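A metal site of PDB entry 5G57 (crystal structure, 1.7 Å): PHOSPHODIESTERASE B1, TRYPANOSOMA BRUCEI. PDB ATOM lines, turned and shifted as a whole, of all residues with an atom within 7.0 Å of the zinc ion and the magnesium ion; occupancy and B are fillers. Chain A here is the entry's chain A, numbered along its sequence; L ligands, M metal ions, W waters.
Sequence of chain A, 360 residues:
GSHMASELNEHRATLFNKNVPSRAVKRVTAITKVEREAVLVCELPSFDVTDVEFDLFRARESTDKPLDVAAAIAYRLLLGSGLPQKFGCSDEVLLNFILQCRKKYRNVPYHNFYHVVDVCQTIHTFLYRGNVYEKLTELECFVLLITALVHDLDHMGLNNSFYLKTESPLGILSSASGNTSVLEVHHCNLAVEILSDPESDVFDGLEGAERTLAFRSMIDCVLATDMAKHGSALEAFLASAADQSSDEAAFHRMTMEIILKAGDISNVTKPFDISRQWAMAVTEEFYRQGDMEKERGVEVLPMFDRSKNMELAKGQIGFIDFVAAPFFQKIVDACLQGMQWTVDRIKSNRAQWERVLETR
Water W6 lies within hydrogen-bond range of O of His 151 (2.7 Å) and OG1 of Thr 225 (2.7 Å).
Water W1 bridges NE2 of His 187 (2.9 Å) and OE2 of Glu 184 (3.3 Å).
Water W3 bridges the side-chain carboxylate (OE2) of Glu 184 and the backbone carbonyl oxygen (O) of Thr 225.
Within 4 Å of the zinc ion: His 115, His 151, Asp 152 and Asp 264.
Within 4 Å of the magnesium ion: Asp 152.
The nearest printed residue that does not touch the magnesium ion is His 187 (4.1 Å).
The magnesium ion is bound by water W1 (2.1 Å), water W3 (2.1 Å), OD1 of Asp 152 (2.1 Å), water W4 (2.1 Å), water W6 (2.1 Å) and water W2 (2.1 Å).
The backbone carbonyl oxygen of Ala 148 sits at hydrogen-bond distance from a ring nitrogen (ND1) of His 151, 2.8 Å away.
The zinc ion is bound by the side-chain carboxylate (OD1) of Asp 264 (2.1 Å), the side-chain carboxylate (OD2) of Asp 152 (2.1 Å), water W2 (2.2 Å), a ring nitrogen (NE2) of His 115 (2.2 Å), a ring nitrogen (NE2) of His 151 (2.2 Å) and water W5 (2.3 Å).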
ATOM      1  N   TYR A 110      13.333   8.275 -16.728  1.00  0.00           N
ATOM      2  CA  TYR A 110      11.933   8.728 -16.499  1.00  0.00           C
ATOM      3  C   TYR A 110      11.260   9.286 -17.777  1.00  0.00           C
ATOM      4  O   TYR A 110      10.185   8.802 -18.174  1.00  0.00           O
ATOM      5  CB  TYR A 110      11.857   9.716 -15.355  1.00  0.00           C
ATOM      6  CG  TYR A 110      10.433  10.146 -15.031  1.00  0.00           C
ATOM      7  CD1 TYR A 110       9.628   9.395 -14.191  1.00  0.00           C
ATOM      8  CD2 TYR A 110       9.912  11.307 -15.562  1.00  0.00           C
ATOM      9  CE1 TYR A 110       8.330   9.771 -13.912  1.00  0.00           C
ATOM     10  CE2 TYR A 110       8.598  11.681 -15.322  1.00  0.00           C
ATOM     11  CZ  TYR A 110       7.821  10.929 -14.487  1.00  0.00           C
ATOM     12  OH  TYR A 110       6.552  11.273 -14.199  1.00  0.00           O
ATOM     13  N   HIS A 111      11.918  10.253 -18.413  1.00  0.00           N
ATOM     14  CA  HIS A 111      11.321  10.978 -19.582  1.00  0.00           C
ATOM     15  C   HIS A 111      11.567  10.246 -20.896  1.00  0.00           C
ATOM     16  O   HIS A 111      12.100  10.809 -21.846  1.00  0.00           O
ATOM     17  CB  HIS A 111      11.819  12.425 -19.637  1.00  0.00           C
ATOM     18  CG  HIS A 111      11.233  13.311 -18.581  1.00  0.00           C
ATOM     19  ND1 HIS A 111      11.940  13.756 -17.490  1.00  0.00           N
ATOM     20  CD2 HIS A 111       9.989  13.806 -18.443  1.00  0.00           C
ATOM     21  CE1 HIS A 111      11.166  14.488 -16.722  1.00  0.00           C
ATOM     22  NE2 HIS A 111       9.970  14.538 -17.281  1.00  0.00           N
ATOM     23  N   HIS A 115       6.777   7.090 -20.152  1.00  0.00           N
ATOM     24  CA  HIS A 115       6.157   8.266 -19.504  1.00  0.00           C
ATOM     25  C   HIS A 115       5.038   8.876 -20.328  1.00  0.00           C
ATOM     26  O   HIS A 115       3.963   9.166 -19.809  1.00  0.00           O
ATOM     27  CB  HIS A 115       7.189   9.302 -19.161  1.00  0.00           C
ATOM     28  CG  HIS A 115       6.615  10.639 -18.760  1.00  0.00           C
ATOM     29  ND1 HIS A 115       5.854  10.843 -17.630  1.00  0.00           N
ATOM     30  CD2 HIS A 115       6.726  11.841 -19.361  1.00  0.00           C
ATOM     31  CE1 HIS A 115       5.498  12.111 -17.574  1.00  0.00           C
ATOM     32  NE2 HIS A 115       6.037  12.747 -18.610  1.00  0.00           N
ATOM     33  N   VAL A 116       5.266   9.064 -21.621  1.00  0.00           N
ATOM     34  CA  VAL A 116       4.211   9.706 -22.454  1.00  0.00           C
ATOM     35  C   VAL A 116       3.032   8.810 -22.738  1.00  0.00           C
ATOM     36  O   VAL A 116       1.882   9.266 -22.821  1.00  0.00           O
ATOM     37  CB  VAL A 116       4.770  10.429 -23.709  1.00  0.00           C
ATOM     38  CG1 VAL A 116       5.870  11.406 -23.337  1.00  0.00           C
ATOM     39  CG2 VAL A 116       5.261   9.467 -24.786  1.00  0.00           C
ATOM     40  N   VAL A 119       1.075   9.065 -19.598  1.00  0.00           N
ATOM     41  CA  VAL A 119       0.276  10.344 -19.548  1.00  0.00           C
ATOM     42  C   VAL A 119      -0.973  10.250 -20.445  1.00  0.00           C
ATOM     43  O   VAL A 119      -2.057  10.674 -20.031  1.00  0.00           O
ATOM     44  CB  VAL A 119       1.177  11.570 -19.863  1.00  0.00           C
ATOM     45  CG1 VAL A 119       0.357  12.848 -20.036  1.00  0.00           C
ATOM     46  CG2 VAL A 119       2.200  11.786 -18.768  1.00  0.00           C
ATOM     47  N   ALA A 148      -0.469  14.301 -25.445  1.00  0.00           N
ATOM     48  CA  ALA A 148       0.233  13.482 -24.465  1.00  0.00           C
ATOM     49  C   ALA A 148       1.462  12.804 -25.057  1.00  0.00           C
ATOM     50  O   ALA A 148       2.502  12.800 -24.427  1.00  0.00           O
ATOM     51  CB  ALA A 148      -0.667  12.436 -23.859  1.00  0.00           C
ATOM     52  N   HIS A 151       4.459  15.507 -25.811  1.00  0.00           N
ATOM     53  CA  HIS A 151       4.710  16.588 -24.879  1.00  0.00           C
ATOM     54  C   HIS A 151       6.130  16.624 -24.275  1.00  0.00           C
ATOM     55  O   HIS A 151       6.522  17.630 -23.704  1.00  0.00           O
ATOM     56  CB  HIS A 151       3.610  16.653 -23.807  1.00  0.00           C
ATOM     57  CG  HIS A 151       3.921  15.829 -22.599  1.00  0.00           C
ATOM     58  ND1 HIS A 151       3.635  14.479 -22.526  1.00  0.00           N
ATOM     59  CD2 HIS A 151       4.534  16.146 -21.443  1.00  0.00           C
ATOM     60  CE1 HIS A 151       4.070  14.003 -21.383  1.00  0.00           C
ATOM     61  NE2 HIS A 151       4.607  14.994 -20.711  1.00  0.00           N
ATOM     62  N   ASP A 152       6.880  15.542 -24.392  1.00  0.00           N
ATOM     63  CA  ASP A 152       8.276  15.482 -23.939  1.00  0.00           C
ATOM     64  C   ASP A 152       9.293  15.016 -25.004  1.00  0.00           C
ATOM     65  O   ASP A 152      10.362  14.548 -24.636  1.00  0.00           O
ATOM     66  CB  ASP A 152       8.394  14.547 -22.694  1.00  0.00           C
ATOM     67  CG  ASP A 152       8.028  15.261 -21.398  1.00  0.00           C
ATOM     68  OD1 ASP A 152       8.313  16.476 -21.220  1.00  0.00           O
ATOM     69  OD2 ASP A 152       7.440  14.603 -20.510  1.00  0.00           O
ATOM     70  N   HIS A 155      13.460  14.545 -24.886  1.00  0.00           N
ATOM     71  CA  HIS A 155      13.943  14.889 -23.574  1.00  0.00           C
ATOM     72  C   HIS A 155      15.221  14.099 -23.335  1.00  0.00           C
ATOM     73  O   HIS A 155      15.263  12.926 -23.651  1.00  0.00           O
ATOM     74  CB  HIS A 155      12.907  14.478 -22.506  1.00  0.00           C
ATOM     75  CG  HIS A 155      12.991  15.272 -21.256  1.00  0.00           C
ATOM     76  ND1 HIS A 155      14.026  15.153 -20.361  1.00  0.00           N
ATOM     77  CD2 HIS A 155      12.137  16.186 -20.725  1.00  0.00           C
ATOM     78  CE1 HIS A 155      13.821  15.957 -19.336  1.00  0.00           C
ATOM     79  NE2 HIS A 155      12.694  16.612 -19.553  1.00  0.00           N
ATOM     80  N   LEU A 183      12.993  23.333 -22.874  1.00  0.00           N
ATOM     81  CA  LEU A 183      12.581  22.028 -23.376  1.00  0.00           C
ATOM     82  C   LEU A 183      11.213  22.072 -24.084  1.00  0.00           C
ATOM     83  O   LEU A 183      11.032  21.396 -25.113  1.00  0.00           O
ATOM     84  CB  LEU A 183      12.503  20.980 -22.267  1.00  0.00           C
ATOM     85  CG  LEU A 183      13.877  20.565 -21.742  1.00  0.00           C
ATOM     86  CD1 LEU A 183      13.691  19.918 -20.393  1.00  0.00           C
ATOM     87  CD2 LEU A 183      14.569  19.632 -22.704  1.00  0.00           C
ATOM     88  N   GLU A 184      10.280  22.824 -23.517  1.00  0.00           N
ATOM     89  CA  GLU A 184       8.905  22.798 -23.985  1.00  0.00           C
ATOM     90  C   GLU A 184       8.816  23.385 -25.385  1.00  0.00           C
ATOM     91  O   GLU A 184       8.166  22.796 -26.259  1.00  0.00           O
ATOM     92  CB  GLU A 184       7.944  23.506 -23.014  1.00  0.00           C
ATOM     93  CG  GLU A 184       7.785  22.770 -21.652  1.00  0.00           C
ATOM     94  CD  GLU A 184       8.973  22.891 -20.708  1.00  0.00           C
ATOM     95  OE1 GLU A 184       9.846  23.790 -20.884  1.00  0.00           O
ATOM     96  OE2 GLU A 184       9.067  22.052 -19.785  1.00  0.00           O
ATOM     97  N   HIS A 187      10.171  20.575 -27.631  1.00  0.00           N
ATOM     98  CA  HIS A 187       9.178  19.542 -27.838  1.00  0.00           C
ATOM     99  C   HIS A 187       8.168  19.987 -28.913  1.00  0.00           C
ATOM    100  O   HIS A 187       7.831  19.200 -29.808  1.00  0.00           O
ATOM    101  CB  HIS A 187       8.394  19.146 -26.554  1.00  0.00           C
ATOM    102  CG  HIS A 187       9.241  18.834 -25.355  1.00  0.00           C
ATOM    103  ND1 HIS A 187      10.388  18.052 -25.416  1.00  0.00           N
ATOM    104  CD2 HIS A 187       9.077  19.175 -24.048  1.00  0.00           C
ATOM    105  CE1 HIS A 187      10.902  17.962 -24.198  1.00  0.00           C
ATOM    106  NE2 HIS A 187      10.104  18.594 -23.355  1.00  0.00           N
ATOM    107  N   VAL A 222       1.451  21.947 -24.324  1.00  0.00           N
ATOM    108  CA  VAL A 222       2.854  21.597 -24.138  1.00  0.00           C
ATOM    109  C   VAL A 222       3.610  22.724 -23.424  1.00  0.00           C
ATOM    110  O   VAL A 222       4.348  22.461 -22.463  1.00  0.00           O
ATOM    111  CB  VAL A 222       3.571  21.210 -25.457  1.00  0.00           C
ATOM    112  CG1 VAL A 222       5.051  20.975 -25.211  1.00  0.00           C
ATOM    113  CG2 VAL A 222       2.926  20.000 -26.083  1.00  0.00           C
ATOM    114  N   THR A 225       3.210  22.829 -19.579  1.00  0.00           N
ATOM    115  CA  THR A 225       3.784  21.778 -18.736  1.00  0.00           C
ATOM    116  C   THR A 225       5.082  22.212 -18.044  1.00  0.00           C
ATOM    117  O   THR A 225       5.585  21.480 -17.196  1.00  0.00           O
ATOM    118  CB  THR A 225       4.029  20.464 -19.506  1.00  0.00           C
ATOM    119  OG1 THR A 225       4.942  20.665 -20.596  1.00  0.00           O
ATOM    120  CG2 THR A 225       2.746  19.903 -19.971  1.00  0.00           C
ATOM    121  N   ASP A 226       5.623  23.388 -18.370  1.00  0.00           N
ATOM    122  CA  ASP A 226       6.787  23.899 -17.648  1.00  0.00           C
ATOM    123  C   ASP A 226       6.401  24.189 -16.186  1.00  0.00           C
ATOM    124  O   ASP A 226       5.587  25.074 -15.926  1.00  0.00           O
ATOM    125  CB  ASP A 226       7.314  25.153 -18.343  1.00  0.00           C
ATOM    126  CG  ASP A 226       8.571  25.736 -17.674  1.00  0.00           C
ATOM    127  OD1 ASP A 226       8.985  25.292 -16.604  1.00  0.00           O
ATOM    128  OD2 ASP A 226       9.130  26.683 -18.260  1.00  0.00           O
ATOM    129  N   LEU A 260      -3.569  18.236 -19.126  1.00  0.00           N
ATOM    130  CA  LEU A 260      -2.239  17.744 -19.468  1.00  0.00           C
ATOM    131  C   LEU A 260      -1.313  17.883 -18.269  1.00  0.00           C
ATOM    132  O   LEU A 260      -0.548  17.021 -18.010  1.00  0.00           O
ATOM    133  CB  LEU A 260      -1.635  18.437 -20.675  1.00  0.00           C
ATOM    134  CG  LEU A 260      -0.249  17.949 -21.090  1.00  0.00           C
ATOM    135  CD1 LEU A 260      -0.167  16.479 -21.391  1.00  0.00           C
ATOM    136  CD2 LEU A 260       0.262  18.718 -22.278  1.00  0.00           C
ATOM    137  N   GLY A 263      -2.082  15.063 -15.889  1.00  0.00           N
ATOM    138  CA  GLY A 263      -1.476  13.821 -16.325  1.00  0.00           C
ATOM    139  C   GLY A 263       0.013  13.778 -16.014  1.00  0.00           C
ATOM    140  O   GLY A 263       0.586  12.741 -15.603  1.00  0.00           O
ATOM    141  N   ASP A 264       0.663  14.890 -16.228  1.00  0.00           N
ATOM    142  CA  ASP A 264       2.086  14.969 -16.011  1.00  0.00           C
ATOM    143  C   ASP A 264       2.478  14.835 -14.515  1.00  0.00           C
ATOM    144  O   ASP A 264       3.571  14.345 -14.227  1.00  0.00           O
ATOM    145  CB  ASP A 264       2.582  16.317 -16.573  1.00  0.00           C
ATOM    146  CG  ASP A 264       3.926  16.253 -17.234  1.00  0.00           C
ATOM    147  OD1 ASP A 264       4.416  15.157 -17.636  1.00  0.00           O
ATOM    148  OD2 ASP A 264       4.463  17.345 -17.394  1.00  0.00           O
ATOM    149  N   ILE A 265       1.636  15.244 -13.567  1.00  0.00           N
ATOM    150  CA  ILE A 265       1.907  15.016 -12.108  1.00  0.00           C
ATOM    151  C   ILE A 265       1.002  13.951 -11.452  1.00  0.00           C
ATOM    152  O   ILE A 265       0.812  13.953 -10.224  1.00  0.00           O
ATOM    153  CB  ILE A 265       1.882  16.341 -11.323  1.00  0.00           C
ATOM    154  CG1 ILE A 265       0.530  17.024 -11.385  1.00  0.00           C
ATOM    155  CG2 ILE A 265       2.940  17.281 -11.853  1.00  0.00           C
ATOM    156  CD1 ILE A 265       0.453  18.214 -10.451  1.00  0.00           C
HETATM  157  C1  LIG L   1       7.636  12.663  -9.045  1.00  0.00           C
HETATM  158  C2  LIG L   1       8.446  13.668  -8.482  1.00  0.00           C
HETATM  159  C3  LIG L   1       9.828  14.436  -6.640  1.00  0.00           C
HETATM  160  C4  LIG L   1      10.144  14.051  -5.211  1.00  0.00           C
HETATM  161  C5  LIG L   1      11.116  14.995  -4.527  1.00  0.00           C
HETATM  162  C6  LIG L   1      10.478  16.024  -3.636  1.00  0.00           C
HETATM  163  C7  LIG L   1       9.219  18.081  -3.860  1.00  0.00           C
HETATM  164  N1  LIG L   1       7.263  23.892  -2.271  1.00  0.00           N
HETATM  165  N2  LIG L   1       7.738  23.569  -1.116  1.00  0.00           N
HETATM  166  N3  LIG L   1       8.251  22.309  -1.153  1.00  0.00           N
HETATM  167  N4  LIG L   1       9.075  17.178 -10.629  1.00  0.00           N
HETATM  168  C8  LIG L   1       9.340  18.367  -2.498  1.00  0.00           C
HETATM  169  C9  LIG L   1       8.433  20.553  -2.895  1.00  0.00           C
HETATM  170  C10 LIG L   1       8.233  19.788  -9.521  1.00  0.00           C
HETATM  171  C11 LIG L   1       6.343  17.649 -14.101  1.00  0.00           C
HETATM  172  O1  LIG L   1       9.421  19.639 -13.171  1.00  0.00           O
HETATM  173  C12 LIG L   1       9.291  18.540 -12.645  1.00  0.00           C
HETATM  174  N5  LIG L   1       9.264  18.378 -11.268  1.00  0.00           N
HETATM  175  C13 LIG L   1       9.490  19.529 -10.364  1.00  0.00           C
HETATM  176  C14 LIG L   1      10.767  19.296  -9.567  1.00  0.00           C
HETATM  177  C15 LIG L   1      11.514  20.554  -9.112  1.00  0.00           C
HETATM  178  C16 LIG L   1      10.719  21.623  -8.348  1.00  0.00           C
HETATM  179  C17 LIG L   1       9.398  21.163  -7.739  1.00  0.00           C
HETATM  180  C18 LIG L   1       8.259  21.087  -8.729  1.00  0.00           C
HETATM  181  C19 LIG L   1       9.080  17.278 -13.454  1.00  0.00           C
HETATM  182  C20 LIG L   1       8.057  16.383 -12.719  1.00  0.00           C
HETATM  183  C21 LIG L   1       6.676  17.053 -12.776  1.00  0.00           C
HETATM  184  C22 LIG L   1       7.248  17.937 -15.013  1.00  0.00           C
HETATM  185  C23 LIG L   1       8.672  17.509 -14.913  1.00  0.00           C
HETATM  186  C24 LIG L   1       8.496  16.222 -11.267  1.00  0.00           C
HETATM  187  C25 LIG L   1       8.199  14.974 -10.518  1.00  0.00           C
HETATM  188  C26 LIG L   1       7.379  13.981 -11.057  1.00  0.00           C
HETATM  189  C27 LIG L   1       7.119  12.825 -10.325  1.00  0.00           C
HETATM  190  O2  LIG L   1       7.407  11.569  -8.250  1.00  0.00           O
HETATM  191  C28 LIG L   1       7.043  10.343  -8.907  1.00  0.00           C
HETATM  192  C29 LIG L   1       8.698  14.819  -9.223  1.00  0.00           C
HETATM  193  O3  LIG L   1       8.937  13.460  -7.213  1.00  0.00           O
HETATM  194  O4  LIG L   1       9.613  16.881  -4.410  1.00  0.00           O
HETATM  195  C30 LIG L   1       8.728  19.036  -4.734  1.00  0.00           C
HETATM  196  C31 LIG L   1       8.351  20.271  -4.245  1.00  0.00           C
HETATM  197  C32 LIG L   1       8.930  19.591  -2.024  1.00  0.00           C
HETATM  198  C33 LIG L   1       8.050  21.871  -2.384  1.00  0.00           C
HETATM  199  N6  LIG L   1       7.467  22.843  -3.091  1.00  0.00           N
HETATM  200 ZN    ZN M   1       5.984  14.919 -18.977  1.00  0.00          ZN
HETATM  201 MG    MG M   2       8.038  18.023 -19.846  1.00  0.00          MG
HETATM  202  O   HOH W   1       9.774  18.912 -20.541  1.00  0.00           O
HETATM  203  O   HOH W   2       6.429  17.023 -18.884  1.00  0.00           O
HETATM  204  O   HOH W   3       7.717  19.756 -18.758  1.00  0.00           O
HETATM  205  O   HOH W   4       9.186  17.288 -18.251  1.00  0.00           O
HETATM  206  O   HOH W   5       7.236  15.148 -17.084  1.00  0.00           O
HETATM  207  O   HOH W   6       6.909  18.955 -21.368  1.00  0.00           O
